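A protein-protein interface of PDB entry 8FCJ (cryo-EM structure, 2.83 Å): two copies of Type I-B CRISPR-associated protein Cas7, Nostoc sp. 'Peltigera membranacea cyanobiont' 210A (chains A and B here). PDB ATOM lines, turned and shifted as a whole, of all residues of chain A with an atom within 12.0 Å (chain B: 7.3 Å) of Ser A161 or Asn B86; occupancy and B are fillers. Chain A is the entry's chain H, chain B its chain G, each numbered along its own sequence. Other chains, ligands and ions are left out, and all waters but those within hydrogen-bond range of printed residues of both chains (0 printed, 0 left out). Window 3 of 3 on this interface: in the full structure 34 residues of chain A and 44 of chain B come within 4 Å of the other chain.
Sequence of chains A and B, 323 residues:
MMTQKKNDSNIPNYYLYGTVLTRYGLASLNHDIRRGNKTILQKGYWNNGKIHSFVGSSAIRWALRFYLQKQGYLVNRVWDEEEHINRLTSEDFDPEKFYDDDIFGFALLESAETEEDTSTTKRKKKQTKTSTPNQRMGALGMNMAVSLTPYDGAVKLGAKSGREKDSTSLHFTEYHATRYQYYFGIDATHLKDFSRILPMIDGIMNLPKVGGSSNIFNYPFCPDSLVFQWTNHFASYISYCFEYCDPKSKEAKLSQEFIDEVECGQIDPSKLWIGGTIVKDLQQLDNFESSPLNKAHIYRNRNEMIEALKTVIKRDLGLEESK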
ATOM      1  N   LYS A 156     -35.530  17.066  26.014  1.00  0.00           N
ATOM      2  CA  LYS A 156     -34.637  15.932  26.183  1.00  0.00           C
ATOM      3  C   LYS A 156     -33.215  16.327  25.817  1.00  0.00           C
ATOM      4  O   LYS A 156     -32.981  17.015  24.820  1.00  0.00           O
ATOM      5  CB  LYS A 156     -35.086  14.739  25.331  1.00  0.00           C
ATOM      6  CG  LYS A 156     -34.129  13.567  25.364  1.00  0.00           C
ATOM      7  CD  LYS A 156     -34.511  12.563  26.425  1.00  0.00           C
ATOM      8  CE  LYS A 156     -33.290  11.817  26.923  1.00  0.00           C
ATOM      9  NZ  LYS A 156     -32.228  11.756  25.885  1.00  0.00           N
ATOM     10  N   LEU A 157     -32.266  15.884  26.636  1.00  0.00           N
ATOM     11  CA  LEU A 157     -30.857  16.117  26.368  1.00  0.00           C
ATOM     12  C   LEU A 157     -30.396  15.282  25.181  1.00  0.00           C
ATOM     13  O   LEU A 157     -30.936  14.209  24.902  1.00  0.00           O
ATOM     14  CB  LEU A 157     -30.016  15.779  27.597  1.00  0.00           C
ATOM     15  CG  LEU A 157     -28.765  16.628  27.797  1.00  0.00           C
ATOM     16  CD1 LEU A 157     -29.105  18.085  27.621  1.00  0.00           C
ATOM     17  CD2 LEU A 157     -28.180  16.384  29.166  1.00  0.00           C
ATOM     18  N   GLY A 158     -29.385  15.783  24.476  1.00  0.00           N
ATOM     19  CA  GLY A 158     -28.927  15.108  23.278  1.00  0.00           C
ATOM     20  C   GLY A 158     -27.427  15.071  23.066  1.00  0.00           C
ATOM     21  O   GLY A 158     -26.968  15.070  21.922  1.00  0.00           O
ATOM     22  N   ALA A 159     -26.648  15.044  24.141  1.00  0.00           N
ATOM     23  CA  ALA A 159     -25.199  15.014  23.995  1.00  0.00           C
ATOM     24  C   ALA A 159     -24.763  13.731  23.298  1.00  0.00           C
ATOM     25  O   ALA A 159     -25.157  12.633  23.696  1.00  0.00           O
ATOM     26  CB  ALA A 159     -24.528  15.129  25.360  1.00  0.00           C
ATOM     27  N   LYS A 160     -23.939  13.869  22.267  1.00  0.00           N
ATOM     28  CA  LYS A 160     -23.479  12.715  21.511  1.00  0.00           C
ATOM     29  C   LYS A 160     -22.238  12.113  22.156  1.00  0.00           C
ATOM     30  O   LYS A 160     -21.436  12.811  22.780  1.00  0.00           O
ATOM     31  CB  LYS A 160     -23.190  13.089  20.057  1.00  0.00           C
ATOM     32  CG  LYS A 160     -21.983  13.979  19.856  1.00  0.00           C
ATOM     33  CD  LYS A 160     -22.117  14.805  18.586  1.00  0.00           C
ATOM     34  CE  LYS A 160     -22.769  14.010  17.468  1.00  0.00           C
ATOM     35  NZ  LYS A 160     -23.168  14.883  16.330  1.00  0.00           N
ATOM     36  N   SER A 161     -22.093  10.800  21.997  1.00  0.00           N
ATOM     37  CA  SER A 161     -21.016  10.073  22.648  1.00  0.00           C
ATOM     38  C   SER A 161     -19.658  10.506  22.113  1.00  0.00           C
ATOM     39  O   SER A 161     -19.514  10.893  20.951  1.00  0.00           O
ATOM     40  CB  SER A 161     -21.194   8.571  22.449  1.00  0.00           C
ATOM     41  OG  SER A 161     -21.522   8.275  21.105  1.00  0.00           O
ATOM     42  N   GLY A 162     -18.653  10.439  22.982  1.00  0.00           N
ATOM     43  CA  GLY A 162     -17.301  10.767  22.586  1.00  0.00           C
ATOM     44  C   GLY A 162     -16.641  11.796  23.476  1.00  0.00           C
ATOM     45  O   GLY A 162     -17.305  12.690  24.008  1.00  0.00           O
ATOM     46  N   ARG A 163     -15.325  11.675  23.648  1.00  0.00           N
ATOM     47  CA  ARG A 163     -14.585  12.661  24.425  1.00  0.00           C
ATOM     48  C   ARG A 163     -14.408  13.961  23.654  1.00  0.00           C
ATOM     49  O   ARG A 163     -14.268  15.028  24.262  1.00  0.00           O
ATOM     50  CB  ARG A 163     -13.226  12.094  24.829  1.00  0.00           C
ATOM     51  CG  ARG A 163     -12.790  12.446  26.238  1.00  0.00           C
ATOM     52  CD  ARG A 163     -11.746  11.464  26.751  1.00  0.00           C
ATOM     53  NE  ARG A 163     -10.894  10.950  25.684  1.00  0.00           N
ATOM     54  CZ  ARG A 163      -9.911  11.630  25.111  1.00  0.00           C
ATOM     55  NH1 ARG A 163      -9.612  12.863  25.486  1.00  0.00           N
ATOM     56  NH2 ARG A 163      -9.209  11.059  24.136  1.00  0.00           N
ATOM     57  N   GLU A 164     -14.410  13.895  22.325  1.00  0.00           N
ATOM     58  CA  GLU A 164     -14.245  15.074  21.477  1.00  0.00           C
ATOM     59  C   GLU A 164     -15.556  15.847  21.477  1.00  0.00           C
ATOM     60  O   GLU A 164     -16.441  15.618  20.652  1.00  0.00           O
ATOM     61  CB  GLU A 164     -13.834  14.669  20.068  1.00  0.00           C
ATOM     62  CG  GLU A 164     -12.368  14.299  19.935  1.00  0.00           C
ATOM     63  CD  GLU A 164     -12.077  13.527  18.665  1.00  0.00           C
ATOM     64  OE1 GLU A 164     -13.027  12.970  18.077  1.00  0.00           O
ATOM     65  OE2 GLU A 164     -10.899  13.477  18.255  1.00  0.00           O
ATOM     66  N   LYS A 165     -15.679  16.782  22.419  1.00  0.00           N
ATOM     67  CA  LYS A 165     -16.909  17.548  22.601  1.00  0.00           C
ATOM     68  C   LYS A 165     -16.774  18.874  21.858  1.00  0.00           C
ATOM     69  O   LYS A 165     -16.400  19.904  22.419  1.00  0.00           O
ATOM     70  CB  LYS A 165     -17.194  17.754  24.085  1.00  0.00           C
ATOM     71  CG  LYS A 165     -18.555  17.253  24.526  1.00  0.00           C
ATOM     72  CD  LYS A 165     -18.586  15.740  24.614  1.00  0.00           C
ATOM     73  CE  LYS A 165     -19.899  15.252  25.197  1.00  0.00           C
ATOM     74  NZ  LYS A 165     -19.863  13.800  25.509  1.00  0.00           N
ATOM     75  N   ASP A 166     -17.082  18.833  20.567  1.00  0.00           N
ATOM     76  CA  ASP A 166     -17.131  20.029  19.743  1.00  0.00           C
ATOM     77  C   ASP A 166     -18.553  20.582  19.746  1.00  0.00           C
ATOM     78  O   ASP A 166     -19.394  20.190  20.558  1.00  0.00           O
ATOM     79  CB  ASP A 166     -16.646  19.724  18.328  1.00  0.00           C
ATOM     80  CG  ASP A 166     -17.584  18.797  17.578  1.00  0.00           C
ATOM     81  OD1 ASP A 166     -18.312  18.021  18.232  1.00  0.00           O
ATOM     82  OD2 ASP A 166     -17.598  18.848  16.331  1.00  0.00           O
ATOM     83  N   SER A 167     -18.840  21.499  18.831  1.00  0.00           N
ATOM     84  CA  SER A 167     -20.203  21.968  18.634  1.00  0.00           C
ATOM     85  C   SER A 167     -21.009  20.854  17.971  1.00  0.00           C
ATOM     86  O   SER A 167     -20.535  19.730  17.786  1.00  0.00           O
ATOM     87  CB  SER A 167     -20.214  23.254  17.816  1.00  0.00           C
ATOM     88  OG  SER A 167     -21.538  23.721  17.635  1.00  0.00           O
ATOM     89  N   THR A 168     -22.257  21.160  17.608  1.00  0.00           N
ATOM     90  CA  THR A 168     -23.193  20.174  17.056  1.00  0.00           C
ATOM     91  C   THR A 168     -23.424  19.020  18.024  1.00  0.00           C
ATOM     92  O   THR A 168     -23.803  17.919  17.619  1.00  0.00           O
ATOM     93  CB  THR A 168     -22.733  19.638  15.696  1.00  0.00           C
ATOM     94  OG1 THR A 168     -21.738  18.626  15.892  1.00  0.00           O
ATOM     95  CG2 THR A 168     -22.158  20.753  14.837  1.00  0.00           C
ATOM     96  N   SER A 169     -23.189  19.265  19.308  1.00  0.00           N
ATOM     97  CA  SER A 169     -23.476  18.317  20.371  1.00  0.00           C
ATOM     98  C   SER A 169     -24.199  19.055  21.486  1.00  0.00           C
ATOM     99  O   SER A 169     -24.260  20.288  21.504  1.00  0.00           O
ATOM    100  CB  SER A 169     -22.199  17.651  20.899  1.00  0.00           C
ATOM    101  OG  SER A 169     -21.276  18.615  21.366  1.00  0.00           O
ATOM    102  N   LEU A 170     -24.756  18.287  22.420  1.00  0.00           N
ATOM    103  CA  LEU A 170     -25.534  18.836  23.527  1.00  0.00           C
ATOM    104  C   LEU A 170     -26.705  19.660  22.985  1.00  0.00           C
ATOM    105  O   LEU A 170     -26.759  20.882  23.110  1.00  0.00           O
ATOM    106  CB  LEU A 170     -24.639  19.657  24.466  1.00  0.00           C
ATOM    107  CG  LEU A 170     -25.082  19.985  25.897  1.00  0.00           C
ATOM    108  CD1 LEU A 170     -25.964  21.218  26.000  1.00  0.00           C
ATOM    109  CD2 LEU A 170     -25.777  18.782  26.503  1.00  0.00           C
ATOM    110  N   HIS A 171     -27.619  18.965  22.317  1.00  0.00           N
ATOM    111  CA  HIS A 171     -28.819  19.583  21.781  1.00  0.00           C
ATOM    112  C   HIS A 171     -30.031  19.202  22.621  1.00  0.00           C
ATOM    113  O   HIS A 171     -30.002  18.248  23.401  1.00  0.00           O
ATOM    114  CB  HIS A 171     -29.047  19.172  20.326  1.00  0.00           C
ATOM    115  CG  HIS A 171     -29.297  17.709  20.139  1.00  0.00           C
ATOM    116  ND1 HIS A 171     -28.288  16.805  19.891  1.00  0.00           N
ATOM    117  CD2 HIS A 171     -30.445  16.993  20.167  1.00  0.00           C
ATOM    118  CE1 HIS A 171     -28.805  15.596  19.765  1.00  0.00           C
ATOM    119  NE2 HIS A 171     -30.112  15.682  19.934  1.00  0.00           N
ATOM    120  N   ILE A 216     -35.964   8.842  17.274  1.00  0.00           N
ATOM    121  CA  ILE A 216     -35.913   9.070  18.709  1.00  0.00           C
ATOM    122  C   ILE A 216     -37.288   8.937  19.349  1.00  0.00           C
ATOM    123  O   ILE A 216     -37.420   8.354  20.425  1.00  0.00           O
ATOM    124  CB  ILE A 216     -35.291  10.453  19.001  1.00  0.00           C
ATOM    125  CG1 ILE A 216     -33.837  10.490  18.539  1.00  0.00           C
ATOM    126  CG2 ILE A 216     -35.346  10.760  20.479  1.00  0.00           C
ATOM    127  CD1 ILE A 216     -33.059   9.232  18.857  1.00  0.00           C
ATOM    128  N   TRP B  62     -27.519   3.541  20.756  1.00  0.00           N
ATOM    129  CA  TRP B  62     -26.083   3.405  20.967  1.00  0.00           C
ATOM    130  C   TRP B  62     -25.734   2.012  21.467  1.00  0.00           C
ATOM    131  O   TRP B  62     -24.723   1.432  21.056  1.00  0.00           O
ATOM    132  CB  TRP B  62     -25.599   4.467  21.954  1.00  0.00           C
ATOM    133  CG  TRP B  62     -24.112   4.655  21.974  1.00  0.00           C
ATOM    134  CD1 TRP B  62     -23.409   5.647  21.364  1.00  0.00           C
ATOM    135  CD2 TRP B  62     -23.149   3.839  22.651  1.00  0.00           C
ATOM    136  NE1 TRP B  62     -22.068   5.497  21.610  1.00  0.00           N
ATOM    137  CE2 TRP B  62     -21.883   4.393  22.398  1.00  0.00           C
ATOM    138  CE3 TRP B  62     -23.235   2.692  23.444  1.00  0.00           C
ATOM    139  CZ2 TRP B  62     -20.714   3.842  22.908  1.00  0.00           C
ATOM    140  CZ3 TRP B  62     -22.073   2.145  23.944  1.00  0.00           C
ATOM    141  CH2 TRP B  62     -20.831   2.721  23.677  1.00  0.00           C
ATOM    142  N   ARG B  65     -25.870  -0.304  18.527  1.00  0.00           N
ATOM    143  CA  ARG B  65     -24.682  -0.093  17.707  1.00  0.00           C
ATOM    144  C   ARG B  65     -23.467  -0.772  18.322  1.00  0.00           C
ATOM    145  O   ARG B  65     -22.676  -1.413  17.619  1.00  0.00           O
ATOM    146  CB  ARG B  65     -24.424   1.403  17.549  1.00  0.00           C
ATOM    147  CG  ARG B  65     -24.771   1.975  16.193  1.00  0.00           C
ATOM    148  CD  ARG B  65     -24.054   3.294  15.988  1.00  0.00           C
ATOM    149  NE  ARG B  65     -24.297   3.862  14.668  1.00  0.00           N
ATOM    150  CZ  ARG B  65     -25.202   4.796  14.417  1.00  0.00           C
ATOM    151  NH1 ARG B  65     -25.976   5.283  15.372  1.00  0.00           N
ATOM    152  NH2 ARG B  65     -25.330   5.258  13.177  1.00  0.00           N
ATOM    153  N   GLN B  69     -21.125  -3.778  16.841  1.00  0.00           N
ATOM    154  CA  GLN B  69     -19.672  -3.673  16.753  1.00  0.00           C
ATOM    155  C   GLN B  69     -18.982  -4.826  17.472  1.00  0.00           C
ATOM    156  O   GLN B  69     -18.036  -5.417  16.942  1.00  0.00           O
ATOM    157  CB  GLN B  69     -19.210  -2.335  17.323  1.00  0.00           C
ATOM    158  CG  GLN B  69     -17.721  -2.264  17.587  1.00  0.00           C
ATOM    159  CD  GLN B  69     -17.305  -0.949  18.200  1.00  0.00           C
ATOM    160  OE1 GLN B  69     -18.072   0.012  18.212  1.00  0.00           O
ATOM    161  NE2 GLN B  69     -16.084  -0.896  18.714  1.00  0.00           N
ATOM    162  N   ARG B  77     -19.291   3.283  12.088  1.00  0.00           N
ATOM    163  CA  ARG B  77     -18.853   4.090  13.225  1.00  0.00           C
ATOM    164  C   ARG B  77     -18.321   3.156  14.304  1.00  0.00           C
ATOM    165  O   ARG B  77     -19.088   2.520  15.029  1.00  0.00           O
ATOM    166  CB  ARG B  77     -19.996   4.954  13.744  1.00  0.00           C
ATOM    167  CG  ARG B  77     -19.725   5.598  15.090  1.00  0.00           C
ATOM    168  CD  ARG B  77     -20.345   6.981  15.187  1.00  0.00           C
ATOM    169  NE  ARG B  77     -21.765   6.949  15.520  1.00  0.00           N
ATOM    170  CZ  ARG B  77     -22.267   6.525  16.672  1.00  0.00           C
ATOM    171  NH1 ARG B  77     -21.492   6.075  17.644  1.00  0.00           N
ATOM    172  NH2 ARG B  77     -23.583   6.558  16.856  1.00  0.00           N
ATOM    173  N   VAL B  78     -17.001   3.079  14.417  1.00  0.00           N
ATOM    174  CA  VAL B  78     -16.352   2.227  15.404  1.00  0.00           C
ATOM    175  C   VAL B  78     -16.085   3.045  16.659  1.00  0.00           C
ATOM    176  O   VAL B  78     -15.533   4.148  16.587  1.00  0.00           O
ATOM    177  CB  VAL B  78     -15.052   1.630  14.844  1.00  0.00           C
ATOM    178  CG1 VAL B  78     -14.223   1.020  15.958  1.00  0.00           C
ATOM    179  CG2 VAL B  78     -15.367   0.594  13.783  1.00  0.00           C
ATOM    180  N   TRP B  79     -16.481   2.507  17.807  1.00  0.00           N
ATOM    181  CA  TRP B  79     -16.338   3.183  19.088  1.00  0.00           C
ATOM    182  C   TRP B  79     -15.104   2.647  19.802  1.00  0.00           C
ATOM    183  O   TRP B  79     -15.008   1.443  20.061  1.00  0.00           O
ATOM    184  CB  TRP B  79     -17.592   2.980  19.938  1.00  0.00           C
ATOM    185  CG  TRP B  79     -17.397   3.212  21.399  1.00  0.00           C
ATOM    186  CD1 TRP B  79     -17.119   2.274  22.348  1.00  0.00           C
ATOM    187  CD2 TRP B  79     -17.488   4.462  22.088  1.00  0.00           C
ATOM    188  NE1 TRP B  79     -17.021   2.863  23.582  1.00  0.00           N
ATOM    189  CE2 TRP B  79     -17.245   4.208  23.448  1.00  0.00           C
ATOM    190  CE3 TRP B  79     -17.749   5.773  21.684  1.00  0.00           C
ATOM    191  CZ2 TRP B  79     -17.253   5.214  24.406  1.00  0.00           C
ATOM    192  CZ3 TRP B  79     -17.757   6.770  22.637  1.00  0.00           C
ATOM    193  CH2 TRP B  79     -17.510   6.486  23.982  1.00  0.00           C
ATOM    194  N   ASP B  80     -14.166   3.537  20.116  1.00  0.00           N
ATOM    195  CA  ASP B  80     -12.944   3.155  20.818  1.00  0.00           C
ATOM    196  C   ASP B  80     -13.228   3.106  22.312  1.00  0.00           C
ATOM    197  O   ASP B  80     -13.462   4.142  22.941  1.00  0.00           O
ATOM    198  CB  ASP B  80     -11.819   4.137  20.511  1.00  0.00           C
ATOM    199  CG  ASP B  80     -10.886   3.633  19.434  1.00  0.00           C
ATOM    200  OD1 ASP B  80     -11.328   2.818  18.598  1.00  0.00           O
ATOM    201  OD2 ASP B  80      -9.710   4.051  19.423  1.00  0.00           O
ATOM    202  N   GLU B  83     -10.265   4.852  24.168  1.00  0.00           N
ATOM    203  CA  GLU B  83     -10.133   6.276  23.892  1.00  0.00           C
ATOM    204  C   GLU B  83     -11.421   7.057  24.104  1.00  0.00           C
ATOM    205  O   GLU B  83     -11.366   8.287  24.195  1.00  0.00           O
ATOM    206  CB  GLU B  83      -9.652   6.497  22.453  1.00  0.00           C
ATOM    207  CG  GLU B  83      -8.210   6.096  22.210  1.00  0.00           C
ATOM    208  CD  GLU B  83      -7.230   7.003  22.923  1.00  0.00           C
ATOM    209  OE1 GLU B  83      -7.487   8.224  22.981  1.00  0.00           O
ATOM    210  OE2 GLU B  83      -6.205   6.497  23.424  1.00  0.00           O
ATOM    211  N   HIS B  84     -12.565   6.376  24.180  1.00  0.00           N
ATOM    212  CA  HIS B  84     -13.866   7.023  24.353  1.00  0.00           C
ATOM    213  C   HIS B  84     -14.131   8.043  23.249  1.00  0.00           C
ATOM    214  O   HIS B  84     -14.612   9.149  23.500  1.00  0.00           O
ATOM    215  CB  HIS B  84     -13.984   7.670  25.734  1.00  0.00           C
ATOM    216  CG  HIS B  84     -14.166   6.684  26.844  1.00  0.00           C
ATOM    217  ND1 HIS B  84     -15.402   6.199  27.214  1.00  0.00           N
ATOM    218  CD2 HIS B  84     -13.268   6.084  27.659  1.00  0.00           C
ATOM    219  CE1 HIS B  84     -15.257   5.347  28.213  1.00  0.00           C
ATOM    220  NE2 HIS B  84     -13.971   5.259  28.501  1.00  0.00           N
ATOM    221  N   ILE B  85     -13.805   7.669  22.011  1.00  0.00           N
ATOM    222  CA  ILE B  85     -14.066   8.494  20.841  1.00  0.00           C
ATOM    223  C   ILE B  85     -14.692   7.623  19.763  1.00  0.00           C
ATOM    224  O   ILE B  85     -14.601   6.396  19.788  1.00  0.00           O
ATOM    225  CB  ILE B  85     -12.794   9.178  20.302  1.00  0.00           C
ATOM    226  CG1 ILE B  85     -11.753   8.131  19.912  1.00  0.00           C
ATOM    227  CG2 ILE B  85     -12.232  10.152  21.321  1.00  0.00           C
ATOM    228  CD1 ILE B  85     -10.706   8.645  18.957  1.00  0.00           C
ATOM    229  N   ASN B  86     -15.336   8.284  18.805  1.00  0.00           N
ATOM    230  CA  ASN B  86     -15.997   7.623  17.690  1.00  0.00           C
ATOM    231  C   ASN B  86     -15.208   7.885  16.416  1.00  0.00           C
ATOM    232  O   ASN B  86     -14.856   9.032  16.126  1.00  0.00           O
ATOM    233  CB  ASN B  86     -17.432   8.122  17.536  1.00  0.00           C
ATOM    234  CG  ASN B  86     -18.433   7.248  18.256  1.00  0.00           C
ATOM    235  OD1 ASN B  86     -18.286   6.029  18.306  1.00  0.00           O
ATOM    236  ND2 ASN B  86     -19.453   7.871  18.829  1.00  0.00           N
ATOM    237  N   ARG B  87     -14.934   6.825  15.661  1.00  0.00           N
ATOM    238  CA  ARG B  87     -14.177   6.929  14.423  1.00  0.00           C
ATOM    239  C   ARG B  87     -14.963   6.290  13.290  1.00  0.00           C
ATOM    240  O   ARG B  87     -15.564   5.227  13.461  1.00  0.00           O
ATOM    241  CB  ARG B  87     -12.809   6.260  14.552  1.00  0.00           C
ATOM    242  CG  ARG B  87     -11.914   6.897  15.595  1.00  0.00           C
ATOM    243  CD  ARG B  87     -10.478   6.976  15.115  1.00  0.00           C
ATOM    244  NE  ARG B  87      -9.537   7.057  16.225  1.00  0.00           N
ATOM    245  CZ  ARG B  87      -9.184   6.029  16.985  1.00  0.00           C
ATOM    246  NH1 ARG B  87      -9.670   4.816  16.776  1.00  0.00           N
ATOM    247  NH2 ARG B  87      -8.321   6.222  17.977  1.00  0.00           N
ATOM    248  N   LEU B  88     -14.951   6.944  12.134  1.00  0.00           N
ATOM    249  CA  LEU B  88     -15.655   6.465  10.952  1.00  0.00           C
ATOM    250  C   LEU B  88     -14.662   5.772  10.029  1.00  0.00           C
ATOM    251  O   LEU B  88     -13.663   6.375   9.622  1.00  0.00           O
ATOM    252  CB  LEU B  88     -16.346   7.618  10.226  1.00  0.00           C
ATOM    253  CG  LEU B  88     -17.650   8.125  10.841  1.00  0.00           C
ATOM    254  CD1 LEU B  88     -18.082   9.416  10.175  1.00  0.00           C
ATOM    255  CD2 LEU B  88     -18.737   7.076  10.722  1.00  0.00           C
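The indole nitrogen of Trp B62 sits at hydrogen-bond distance from the side-chain hydroxyl of Ser A161, 2.9 Å away. The side-chain carboxylate of Glu B83 lies within salt-bridge range of the guanidinium group of Arg A163, at 3.5 Å. The backbone NH (N) of Arg A163 sits at hydrogen-bond distance from the backbone carbonyl oxygen (O) of His B84. ND2 of Asn B86 sits at hydrogen-bond distance from OG of Ser A161, at 3.1 Å.
Of the 17 printed residues of chain A, 3 touch a printed residue of chain B. Of the 13 printed residues of chain B, 5 touch a printed residue of chain A. Hydrophobic or aromatic side chains of chain B within 4 Å of the printed part of chain A: Trp B62 and Trp B79. Among the printed residues, 7 pairs touch across the chains. Among the printed residues, Asp or Glu carboxylates within 4 Å of a Lys or Arg side-chain nitrogen of the other chain: Arg A163 with Glu B83.
Leu A157 touches none of the printed residues of chain B. Printed residues of chain B within 4 Å of Ser A161: Trp B62 (2.9 Å), Trp B79 (3.9 Å) and Asn B86 (3.1 Å). Printed residues of chain B within 4 Å of Arg A163: Glu B83 and His B84. Glu A164 touches none of the printed residues of chain B. Of chain A, only Ser A161 (2.9 Å) comes within 4 Å of Trp B62. No residue of chain A comes within 4 Å of Arg B77. Val B78 touches none of the printed residues of chain A. Of chain A, only Ser A161 and Gly A162 come within 4 Å of Trp B79. No residue of chain A comes within 4 Å of Asp B80. Printed residues of chain A within 4 Å of His B84: Gly A162 (3.3 Å) and Arg A163 (2.6 Å). Ile B85 touches none of the printed residues of chain A. Asn B86 touches just one residue of chain A: Ser A161. No residue of chain A comes within 4 Å of Arg B87. Leu B88 touches none of the printed residues of chain A. The nearest residue of chain B that does not touch Ser A161 is Arg B77 (4.1 Å).
Among the printed residues, pairs that only touch across the chains: Ser A161 with Trp B79, Gly A162 with Trp B79 and Gly A162 with His B84.
No position is printed for both chains.
The side-chain amide nitrogen of Gln B69 sits at hydrogen-bond distance from the backbone carbonyl oxygen of Trp B79 (2.9 Å). The guanidinium group (NH1) of Arg B77 lies close to the side-chain amide nitrogen (ND2) of Asn B86 (3.0 Å). The side-chain amino group of Lys A165 is in hydrogen-bond range of the backbone carbonyl oxygen of Gly A162 (3.2 Å).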
